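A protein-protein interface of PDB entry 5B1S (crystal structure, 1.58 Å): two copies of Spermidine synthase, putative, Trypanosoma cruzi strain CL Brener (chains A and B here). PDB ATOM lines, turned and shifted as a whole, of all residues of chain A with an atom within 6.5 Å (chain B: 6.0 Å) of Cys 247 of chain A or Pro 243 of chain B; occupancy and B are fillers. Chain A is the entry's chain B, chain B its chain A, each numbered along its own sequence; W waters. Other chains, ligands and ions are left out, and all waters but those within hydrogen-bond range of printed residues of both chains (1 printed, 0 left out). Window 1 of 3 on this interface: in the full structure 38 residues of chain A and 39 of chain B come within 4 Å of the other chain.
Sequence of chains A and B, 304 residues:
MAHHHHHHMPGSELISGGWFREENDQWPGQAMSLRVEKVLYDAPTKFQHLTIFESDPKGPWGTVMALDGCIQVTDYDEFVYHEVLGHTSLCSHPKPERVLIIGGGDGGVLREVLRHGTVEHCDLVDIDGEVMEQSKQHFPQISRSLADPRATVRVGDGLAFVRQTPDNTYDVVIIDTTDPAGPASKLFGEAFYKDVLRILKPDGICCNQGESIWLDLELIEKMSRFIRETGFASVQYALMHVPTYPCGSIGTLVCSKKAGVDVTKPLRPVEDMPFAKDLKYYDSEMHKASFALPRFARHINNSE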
ATOM      1  N   TRP A  27      -8.224   9.849  -4.332  1.00  0.00           N
ATOM      2  CA  TRP A  27      -8.094   8.466  -4.787  1.00  0.00           C
ATOM      3  C   TRP A  27      -7.450   8.395  -6.154  1.00  0.00           C
ATOM      4  O   TRP A  27      -8.103   8.133  -7.143  1.00  0.00           O
ATOM      5  CB  TRP A  27      -9.477   7.717  -4.753  1.00  0.00           C
ATOM      6  CG  TRP A  27     -10.645   8.511  -5.131  1.00  0.00           C
ATOM      7  CD1 TRP A  27     -11.148   8.703  -6.386  1.00  0.00           C
ATOM      8  CD2 TRP A  27     -11.524   9.182  -4.240  1.00  0.00           C
ATOM      9  NE1 TRP A  27     -12.257   9.502  -6.333  1.00  0.00           N
ATOM     10  CE2 TRP A  27     -12.528   9.777  -5.019  1.00  0.00           C
ATOM     11  CE3 TRP A  27     -11.547   9.339  -2.874  1.00  0.00           C
ATOM     12  CZ2 TRP A  27     -13.538  10.600  -4.480  1.00  0.00           C
ATOM     13  CZ3 TRP A  27     -12.531  10.136  -2.343  1.00  0.00           C
ATOM     14  CH2 TRP A  27     -13.496  10.769  -3.135  1.00  0.00           C
ATOM     15  N   GLN A  30      -8.022   6.155 -10.051  1.00  0.00           N
ATOM     16  CA  GLN A  30      -9.247   5.445 -10.251  1.00  0.00           C
ATOM     17  C   GLN A  30     -10.419   6.396 -10.259  1.00  0.00           C
ATOM     18  O   GLN A  30     -10.380   7.473  -9.604  1.00  0.00           O
ATOM     19  CB  GLN A  30      -9.486   4.426  -9.109  1.00  0.00           C
ATOM     20  CG  GLN A  30      -9.706   5.126  -7.728  1.00  0.00           C
ATOM     21  CD  GLN A  30      -9.650   4.195  -6.572  1.00  0.00           C
ATOM     22  OE1 GLN A  30      -8.552   3.815  -6.069  1.00  0.00           O
ATOM     23  NE2 GLN A  30     -10.867   3.817  -6.037  1.00  0.00           N
ATOM     24  N   SER A 212     -12.194   4.909   4.259  1.00  0.00           N
ATOM     25  CA  SER A 212     -12.038   3.591   3.625  1.00  0.00           C
ATOM     26  C   SER A 212     -10.875   2.780   4.125  1.00  0.00           C
ATOM     27  O   SER A 212      -9.793   3.341   4.284  1.00  0.00           O
ATOM     28  CB  SER A 212     -11.737   3.858   2.137  1.00  0.00           C
ATOM     29  OG  SER A 212     -11.378   2.655   1.457  1.00  0.00           O
ATOM     30  N   TRP A 214      -9.300   0.734   2.365  1.00  0.00           N
ATOM     31  CA  TRP A 214      -8.522   0.530   1.134  1.00  0.00           C
ATOM     32  C   TRP A 214      -7.668   1.718   0.783  1.00  0.00           C
ATOM     33  O   TRP A 214      -6.560   1.569   0.229  1.00  0.00           O
ATOM     34  CB  TRP A 214      -9.394   0.161  -0.104  1.00  0.00           C
ATOM     35  CG  TRP A 214     -10.070  -1.142   0.088  1.00  0.00           C
ATOM     36  CD1 TRP A 214     -11.434  -1.343   0.427  1.00  0.00           C
ATOM     37  CD2 TRP A 214      -9.502  -2.428  -0.067  1.00  0.00           C
ATOM     38  NE1 TRP A 214     -11.676  -2.682   0.503  1.00  0.00           N
ATOM     39  CE2 TRP A 214     -10.516  -3.370   0.245  1.00  0.00           C
ATOM     40  CE3 TRP A 214      -8.211  -2.902  -0.422  1.00  0.00           C
ATOM     41  CZ2 TRP A 214     -10.301  -4.749   0.193  1.00  0.00           C
ATOM     42  CZ3 TRP A 214      -7.975  -4.286  -0.450  1.00  0.00           C
ATOM     43  CH2 TRP A 214      -9.042  -5.197  -0.194  1.00  0.00           C
ATOM     44  N   LEU A 215      -8.178   2.894   1.128  1.00  0.00           N
ATOM     45  CA  LEU A 215      -7.583   4.191   0.676  1.00  0.00           C
ATOM     46  C   LEU A 215      -7.064   4.967   1.849  1.00  0.00           C
ATOM     47  O   LEU A 215      -6.143   5.804   1.668  1.00  0.00           O
ATOM     48  CB  LEU A 215      -8.663   5.021  -0.072  1.00  0.00           C
ATOM     49  CG  LEU A 215      -9.261   4.452  -1.346  1.00  0.00           C
ATOM     50  CD1 LEU A 215     -10.539   5.183  -1.725  1.00  0.00           C
ATOM     51  CD2 LEU A 215      -8.232   4.549  -2.465  1.00  0.00           C
ATOM     52  N   VAL A 242     -21.142  -0.138   0.228  1.00  0.00           N
ATOM     53  CA  VAL A 242     -21.810   0.971  -0.460  1.00  0.00           C
ATOM     54  C   VAL A 242     -21.158   1.144  -1.848  1.00  0.00           C
ATOM     55  O   VAL A 242     -20.048   1.582  -1.964  1.00  0.00           O
ATOM     56  CB  VAL A 242     -21.659   2.353   0.217  1.00  0.00           C
ATOM     57  CG1 VAL A 242     -22.532   3.360  -0.556  1.00  0.00           C
ATOM     58  CG2 VAL A 242     -22.174   2.269   1.664  1.00  0.00           C
ATOM     59  N   PRO A 243     -21.828   0.637  -2.857  1.00  0.00           N
ATOM     60  CA  PRO A 243     -21.195   0.638  -4.205  1.00  0.00           C
ATOM     61  C   PRO A 243     -20.676   1.950  -4.672  1.00  0.00           C
ATOM     62  O   PRO A 243     -19.644   1.997  -5.363  1.00  0.00           O
ATOM     63  CB  PRO A 243     -22.324   0.121  -5.123  1.00  0.00           C
ATOM     64  CG  PRO A 243     -23.098  -0.855  -4.235  1.00  0.00           C
ATOM     65  CD  PRO A 243     -23.079  -0.177  -2.869  1.00  0.00           C
ATOM     66  N   TYR A 245     -19.535   4.620  -2.978  1.00  0.00           N
ATOM     67  CA  TYR A 245     -18.404   5.322  -2.369  1.00  0.00           C
ATOM     68  C   TYR A 245     -17.141   4.630  -2.900  1.00  0.00           C
ATOM     69  O   TYR A 245     -17.178   3.449  -3.331  1.00  0.00           O
ATOM     70  CB  TYR A 245     -18.475   5.292  -0.809  1.00  0.00           C
ATOM     71  CG  TYR A 245     -19.634   6.048  -0.299  1.00  0.00           C
ATOM     72  CD1 TYR A 245     -19.967   7.289  -0.806  1.00  0.00           C
ATOM     73  CD2 TYR A 245     -20.348   5.597   0.821  1.00  0.00           C
ATOM     74  CE1 TYR A 245     -21.012   8.028  -0.273  1.00  0.00           C
ATOM     75  CE2 TYR A 245     -21.410   6.318   1.370  1.00  0.00           C
ATOM     76  CZ  TYR A 245     -21.713   7.545   0.852  1.00  0.00           C
ATOM     77  OH  TYR A 245     -22.800   8.259   1.277  1.00  0.00           O
ATOM     78  N   PRO A 246     -16.034   5.379  -2.896  1.00  0.00           N
ATOM     79  CA  PRO A 246     -14.776   4.861  -3.549  1.00  0.00           C
ATOM     80  C   PRO A 246     -14.324   3.506  -2.947  1.00  0.00           C
ATOM     81  O   PRO A 246     -14.301   3.276  -1.692  1.00  0.00           O
ATOM     82  CB  PRO A 246     -13.782   5.962  -3.321  1.00  0.00           C
ATOM     83  CG  PRO A 246     -14.623   7.215  -3.128  1.00  0.00           C
ATOM     84  CD  PRO A 246     -15.894   6.757  -2.356  1.00  0.00           C
ATOM     85  N   CYS A 247     -14.158   2.578  -3.865  1.00  0.00           N
ATOM     86  CA  CYS A 247     -13.748   1.184  -3.621  1.00  0.00           C
ATOM     87  C   CYS A 247     -14.863   0.323  -3.077  1.00  0.00           C
ATOM     88  O   CYS A 247     -14.625  -0.867  -2.784  1.00  0.00           O
ATOM     89  CB  CYS A 247     -12.590   0.988  -2.676  1.00  0.00           C
ATOM     90  SG  CYS A 247     -10.962   1.686  -3.215  1.00  0.00           S
ATOM     91  N   GLY A 248     -16.055   0.903  -2.994  1.00  0.00           N
ATOM     92  CA  GLY A 248     -17.287   0.091  -2.702  1.00  0.00           C
ATOM     93  C   GLY A 248     -17.554  -0.146  -1.242  1.00  0.00           C
ATOM     94  O   GLY A 248     -18.437  -0.987  -0.925  1.00  0.00           O
ATOM     95  N   SER A 249     -16.923   0.603  -0.371  1.00  0.00           N
ATOM     96  CA  SER A 249     -17.276   0.510   1.031  1.00  0.00           C
ATOM     97  C   SER A 249     -16.956   1.823   1.749  1.00  0.00           C
ATOM     98  O   SER A 249     -16.286   2.713   1.107  1.00  0.00           O
ATOM     99  CB  SER A 249     -16.606  -0.703   1.686  1.00  0.00           C
ATOM    100  OG  SER A 249     -15.174  -0.488   1.793  1.00  0.00           O
ATOM    101  N   MET B  32     -16.307   1.168 -13.630  1.00  0.00           N
ATOM    102  CA  MET B  32     -15.135   1.471 -12.962  1.00  0.00           C
ATOM    103  C   MET B  32     -14.068   1.832 -13.978  1.00  0.00           C
ATOM    104  O   MET B  32     -14.002   1.227 -15.009  1.00  0.00           O
ATOM    105  CB  MET B  32     -14.690   0.257 -12.140  1.00  0.00           C
ATOM    106  CG  MET B  32     -13.367   0.491 -11.400  1.00  0.00           C
ATOM    107  SD  MET B  32     -13.544   1.913 -10.288  1.00  0.00           S
ATOM    108  CE  MET B  32     -12.113   1.687  -9.253  1.00  0.00           C
ATOM    109  N   TRP B  61      -3.217   0.029  -7.368  1.00  0.00           N
ATOM    110  CA  TRP B  61      -3.794  -1.171  -8.069  1.00  0.00           C
ATOM    111  C   TRP B  61      -2.780  -2.049  -8.743  1.00  0.00           C
ATOM    112  O   TRP B  61      -2.964  -3.241  -8.823  1.00  0.00           O
ATOM    113  CB  TRP B  61      -4.908  -0.747  -9.011  1.00  0.00           C
ATOM    114  CG  TRP B  61      -5.919   0.048  -8.172  1.00  0.00           C
ATOM    115  CD1 TRP B  61      -6.102   1.414  -8.154  1.00  0.00           C
ATOM    116  CD2 TRP B  61      -6.803  -0.478  -7.140  1.00  0.00           C
ATOM    117  NE1 TRP B  61      -7.048   1.749  -7.230  1.00  0.00           N
ATOM    118  CE2 TRP B  61      -7.507   0.617  -6.604  1.00  0.00           C
ATOM    119  CE3 TRP B  61      -7.102  -1.766  -6.692  1.00  0.00           C
ATOM    120  CZ2 TRP B  61      -8.449   0.472  -5.540  1.00  0.00           C
ATOM    121  CZ3 TRP B  61      -8.036  -1.913  -5.699  1.00  0.00           C
ATOM    122  CH2 TRP B  61      -8.675  -0.802  -5.099  1.00  0.00           C
ATOM    123  N   ASP B  77      -5.766  -6.054  -4.731  1.00  0.00           N
ATOM    124  CA  ASP B  77      -6.877  -6.700  -3.988  1.00  0.00           C
ATOM    125  C   ASP B  77      -7.147  -8.157  -4.361  1.00  0.00           C
ATOM    126  O   ASP B  77      -8.164  -8.709  -3.856  1.00  0.00           O
ATOM    127  CB  ASP B  77      -8.216  -5.914  -4.165  1.00  0.00           C
ATOM    128  CG  ASP B  77      -8.673  -5.811  -5.544  1.00  0.00           C
ATOM    129  OD1 ASP B  77      -8.097  -6.408  -6.462  1.00  0.00           O
ATOM    130  OD2 ASP B  77      -9.670  -5.109  -5.829  1.00  0.00           O
ATOM    131  N   VAL B  80      -8.291 -11.105  -1.811  1.00  0.00           N
ATOM    132  CA  VAL B  80      -9.588 -11.272  -1.091  1.00  0.00           C
ATOM    133  C   VAL B  80     -10.333 -12.495  -1.697  1.00  0.00           C
ATOM    134  O   VAL B  80     -10.634 -13.462  -1.012  1.00  0.00           O
ATOM    135  CB  VAL B  80     -10.499 -10.031  -1.270  1.00  0.00           C
ATOM    136  CG1 VAL B  80     -11.812 -10.303  -0.491  1.00  0.00           C
ATOM    137  CG2 VAL B  80      -9.823  -8.805  -0.638  1.00  0.00           C
ATOM    138  N   HIS B 241     -15.548  -8.266   0.143  1.00  0.00           N
ATOM    139  CA  HIS B 241     -15.252  -6.876  -0.281  1.00  0.00           C
ATOM    140  C   HIS B 241     -14.124  -6.914  -1.346  1.00  0.00           C
ATOM    141  O   HIS B 241     -12.939  -7.315  -0.971  1.00  0.00           O
ATOM    142  CB  HIS B 241     -14.681  -6.209   0.935  1.00  0.00           C
ATOM    143  CG  HIS B 241     -15.749  -5.761   1.875  1.00  0.00           C
ATOM    144  ND1 HIS B 241     -16.169  -6.486   2.973  1.00  0.00           N
ATOM    145  CD2 HIS B 241     -16.424  -4.580   1.897  1.00  0.00           C
ATOM    146  CE1 HIS B 241     -17.130  -5.794   3.592  1.00  0.00           C
ATOM    147  NE2 HIS B 241     -17.293  -4.654   2.960  1.00  0.00           N
ATOM    148  N   VAL B 242     -14.463  -6.614  -2.621  1.00  0.00           N
ATOM    149  CA  VAL B 242     -13.436  -6.574  -3.682  1.00  0.00           C
ATOM    150  C   VAL B 242     -13.655  -5.283  -4.479  1.00  0.00           C
ATOM    151  O   VAL B 242     -14.609  -5.191  -5.288  1.00  0.00           O
ATOM    152  CB  VAL B 242     -13.460  -7.799  -4.615  1.00  0.00           C
ATOM    153  CG1 VAL B 242     -12.338  -7.659  -5.672  1.00  0.00           C
ATOM    154  CG2 VAL B 242     -13.418  -9.108  -3.843  1.00  0.00           C
ATOM    155  N   PRO B 243     -12.821  -4.260  -4.230  1.00  0.00           N
ATOM    156  CA  PRO B 243     -13.069  -2.966  -4.841  1.00  0.00           C
ATOM    157  C   PRO B 243     -13.167  -3.031  -6.396  1.00  0.00           C
ATOM    158  O   PRO B 243     -13.945  -2.271  -7.007  1.00  0.00           O
ATOM    159  CB  PRO B 243     -11.815  -2.202  -4.441  1.00  0.00           C
ATOM    160  CG  PRO B 243     -11.552  -2.620  -3.066  1.00  0.00           C
ATOM    161  CD  PRO B 243     -11.766  -4.138  -3.199  1.00  0.00           C
ATOM    162  N   THR B 244     -12.420  -3.923  -7.002  1.00  0.00           N
ATOM    163  CA  THR B 244     -12.312  -3.894  -8.465  1.00  0.00           C
ATOM    164  C   THR B 244     -13.231  -4.882  -9.152  1.00  0.00           C
ATOM    165  O   THR B 244     -13.003  -5.252 -10.284  1.00  0.00           O
ATOM    166  CB  THR B 244     -10.832  -4.059  -8.933  1.00  0.00           C
ATOM    167  OG1 THR B 244     -10.317  -5.244  -8.392  1.00  0.00           O
ATOM    168  CG2 THR B 244     -10.001  -2.884  -8.335  1.00  0.00           C
ATOM    169  N   TYR B 245     -14.229  -5.439  -8.416  1.00  0.00           N
ATOM    170  CA  TYR B 245     -15.330  -6.092  -9.088  1.00  0.00           C
ATOM    171  C   TYR B 245     -16.549  -5.174  -9.039  1.00  0.00           C
ATOM    172  O   TYR B 245     -16.560  -4.298  -8.201  1.00  0.00           O
ATOM    173  CB  TYR B 245     -15.665  -7.499  -8.481  1.00  0.00           C
ATOM    174  CG  TYR B 245     -14.573  -8.499  -8.642  1.00  0.00           C
ATOM    175  CD1 TYR B 245     -13.881  -8.584  -9.876  1.00  0.00           C
ATOM    176  CD2 TYR B 245     -14.334  -9.397  -7.680  1.00  0.00           C
ATOM    177  CE1 TYR B 245     -12.854  -9.577 -10.064  1.00  0.00           C
ATOM    178  CE2 TYR B 245     -13.334 -10.365  -7.837  1.00  0.00           C
ATOM    179  CZ  TYR B 245     -12.664 -10.466  -9.053  1.00  0.00           C
ATOM    180  OH  TYR B 245     -11.659 -11.411  -9.168  1.00  0.00           O
ATOM    181  N   PRO B 246     -17.472  -5.326  -9.997  1.00  0.00           N
ATOM    182  CA  PRO B 246     -18.530  -4.343 -10.144  1.00  0.00           C
ATOM    183  C   PRO B 246     -19.358  -4.168  -8.897  1.00  0.00           C
ATOM    184  O   PRO B 246     -19.725  -5.136  -8.281  1.00  0.00           O
ATOM    185  CB  PRO B 246     -19.334  -4.896 -11.303  1.00  0.00           C
ATOM    186  CG  PRO B 246     -18.219  -5.478 -12.201  1.00  0.00           C
ATOM    187  CD  PRO B 246     -17.409  -6.239 -11.162  1.00  0.00           C
ATOM    188  N   CYS B 247     -19.509  -2.921  -8.511  1.00  0.00           N
ATOM    189  CA  CYS B 247     -20.118  -2.510  -7.254  1.00  0.00           C
ATOM    190  C   CYS B 247     -19.304  -2.727  -5.996  1.00  0.00           C
ATOM    191  O   CYS B 247     -19.828  -2.427  -4.908  1.00  0.00           O
ATOM    192  CB  CYS B 247     -21.509  -3.064  -7.101  1.00  0.00           C
ATOM    193  SG  CYS B 247     -22.785  -2.601  -8.293  1.00  0.00           S
ATOM    194  N   GLY B 248     -18.099  -3.306  -6.088  1.00  0.00           N
ATOM    195  CA  GLY B 248     -17.204  -3.388  -4.935  1.00  0.00           C
ATOM    196  C   GLY B 248     -17.360  -4.675  -4.138  1.00  0.00           C
ATOM    197  O   GLY B 248     -16.883  -4.710  -3.018  1.00  0.00           O
ATOM    198  N   SER B 249     -18.117  -5.624  -4.666  1.00  0.00           N
ATOM    199  CA  SER B 249     -18.159  -6.884  -3.999  1.00  0.00           C
ATOM    200  C   SER B 249     -18.427  -7.992  -4.964  1.00  0.00           C
ATOM    201  O   SER B 249     -18.796  -7.780  -6.122  1.00  0.00           O
ATOM    202  CB  SER B 249     -19.207  -6.842  -2.892  1.00  0.00           C
ATOM    203  OG  SER B 249     -20.549  -6.726  -3.455  1.00  0.00           O
HETATM  204  O   HOH W   1     -14.869  -3.285  -1.672  1.00  0.00           O
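NE1 of Trp 61 of chain B lies within hydrogen-bond range of OE1 of Gln 30 of chain A, 2.8 Å away.
The side-chain sulfur (SG) of Cys 247 of chain A is in hydrogen-bond range of the side-chain amide nitrogen (NE2) of Gln 30 of chain A, 3.5 Å away. The side-chain hydroxyl (OG) of Ser 212 of chain A lies within hydrogen-bond range of the backbone NH (N) of Trp 214 of chain A, 3.0 Å away.
Among the printed residues, pairs that only touch across the chains: Gln 30 of chain A with Met 32 of chain B, Trp 214 of chain A with Val 80 of chain B, Trp 214 of chain A with His 241 of chain B, Trp 214 of chain A with Pro 243 of chain B, Pro 243 of chain A with Cys 247 of chain B, Cys 247 of chain A with Trp 61 of chain B, Cys 247 of chain A with Pro 243 of chain B and Ser 249 of chain A with His 241 of chain B.
Of the printed residues of chain B, Pro 243 of chain A touches Cys 247. Pro 246 of chain A touches none of the printed residues of chain B. Of chain B, only Trp 61 (3.6 Å) and Pro 243 (3.3 Å) come within 4 Å of Cys 247 of chain A. Printed residues of chain A within 4 Å of Met 32 of chain B: Gln 30 (3.8 Å). Of the printed residues of chain A, Val 80 of chain B touches Trp 214. Of the printed residues of chain A, His 241 of chain B touches Trp 214 and Ser 249. Pro 243 of chain B touches just these residues of chain A: Trp 214 (3.5 Å) and Cys 247 (3.3 Å). The nearest residue of chain B that does not touch Cys 247 of chain A is Gly 248 of chain B (4.2 Å).
Of the 12 printed residues of chain A, 5 touch a printed residue of chain B. Of the 13 printed residues of chain B, 6 touch a printed residue of chain A. Hydrophobic or aromatic side chains of chain B that line the printed part of chain A: Met 32, Trp 61, Val 80, His 241 and Pro 243. Among the printed residues, 9 pairs touch across the chains. Among the printed residues, no Asp or Glu carboxylate lies within 4 Å of a Lys or Arg side-chain nitrogen of the other chain.
Pro 243 of chain A touches Cys 247 of chain B, and with the chains exchanged Cys 247 of chain A touches Pro 243 of chain B. Of the 9 pairs that touch across the chains among the printed residues, 2 have their exchanged pair printed and touching as well.
Water W1 lies within hydrogen-bond range of O of Cys 247 of chain A (2.7 Å), O of Gly 248 of chain B (2.8 Å) and N of Val 242 of chain B (3.5 Å).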
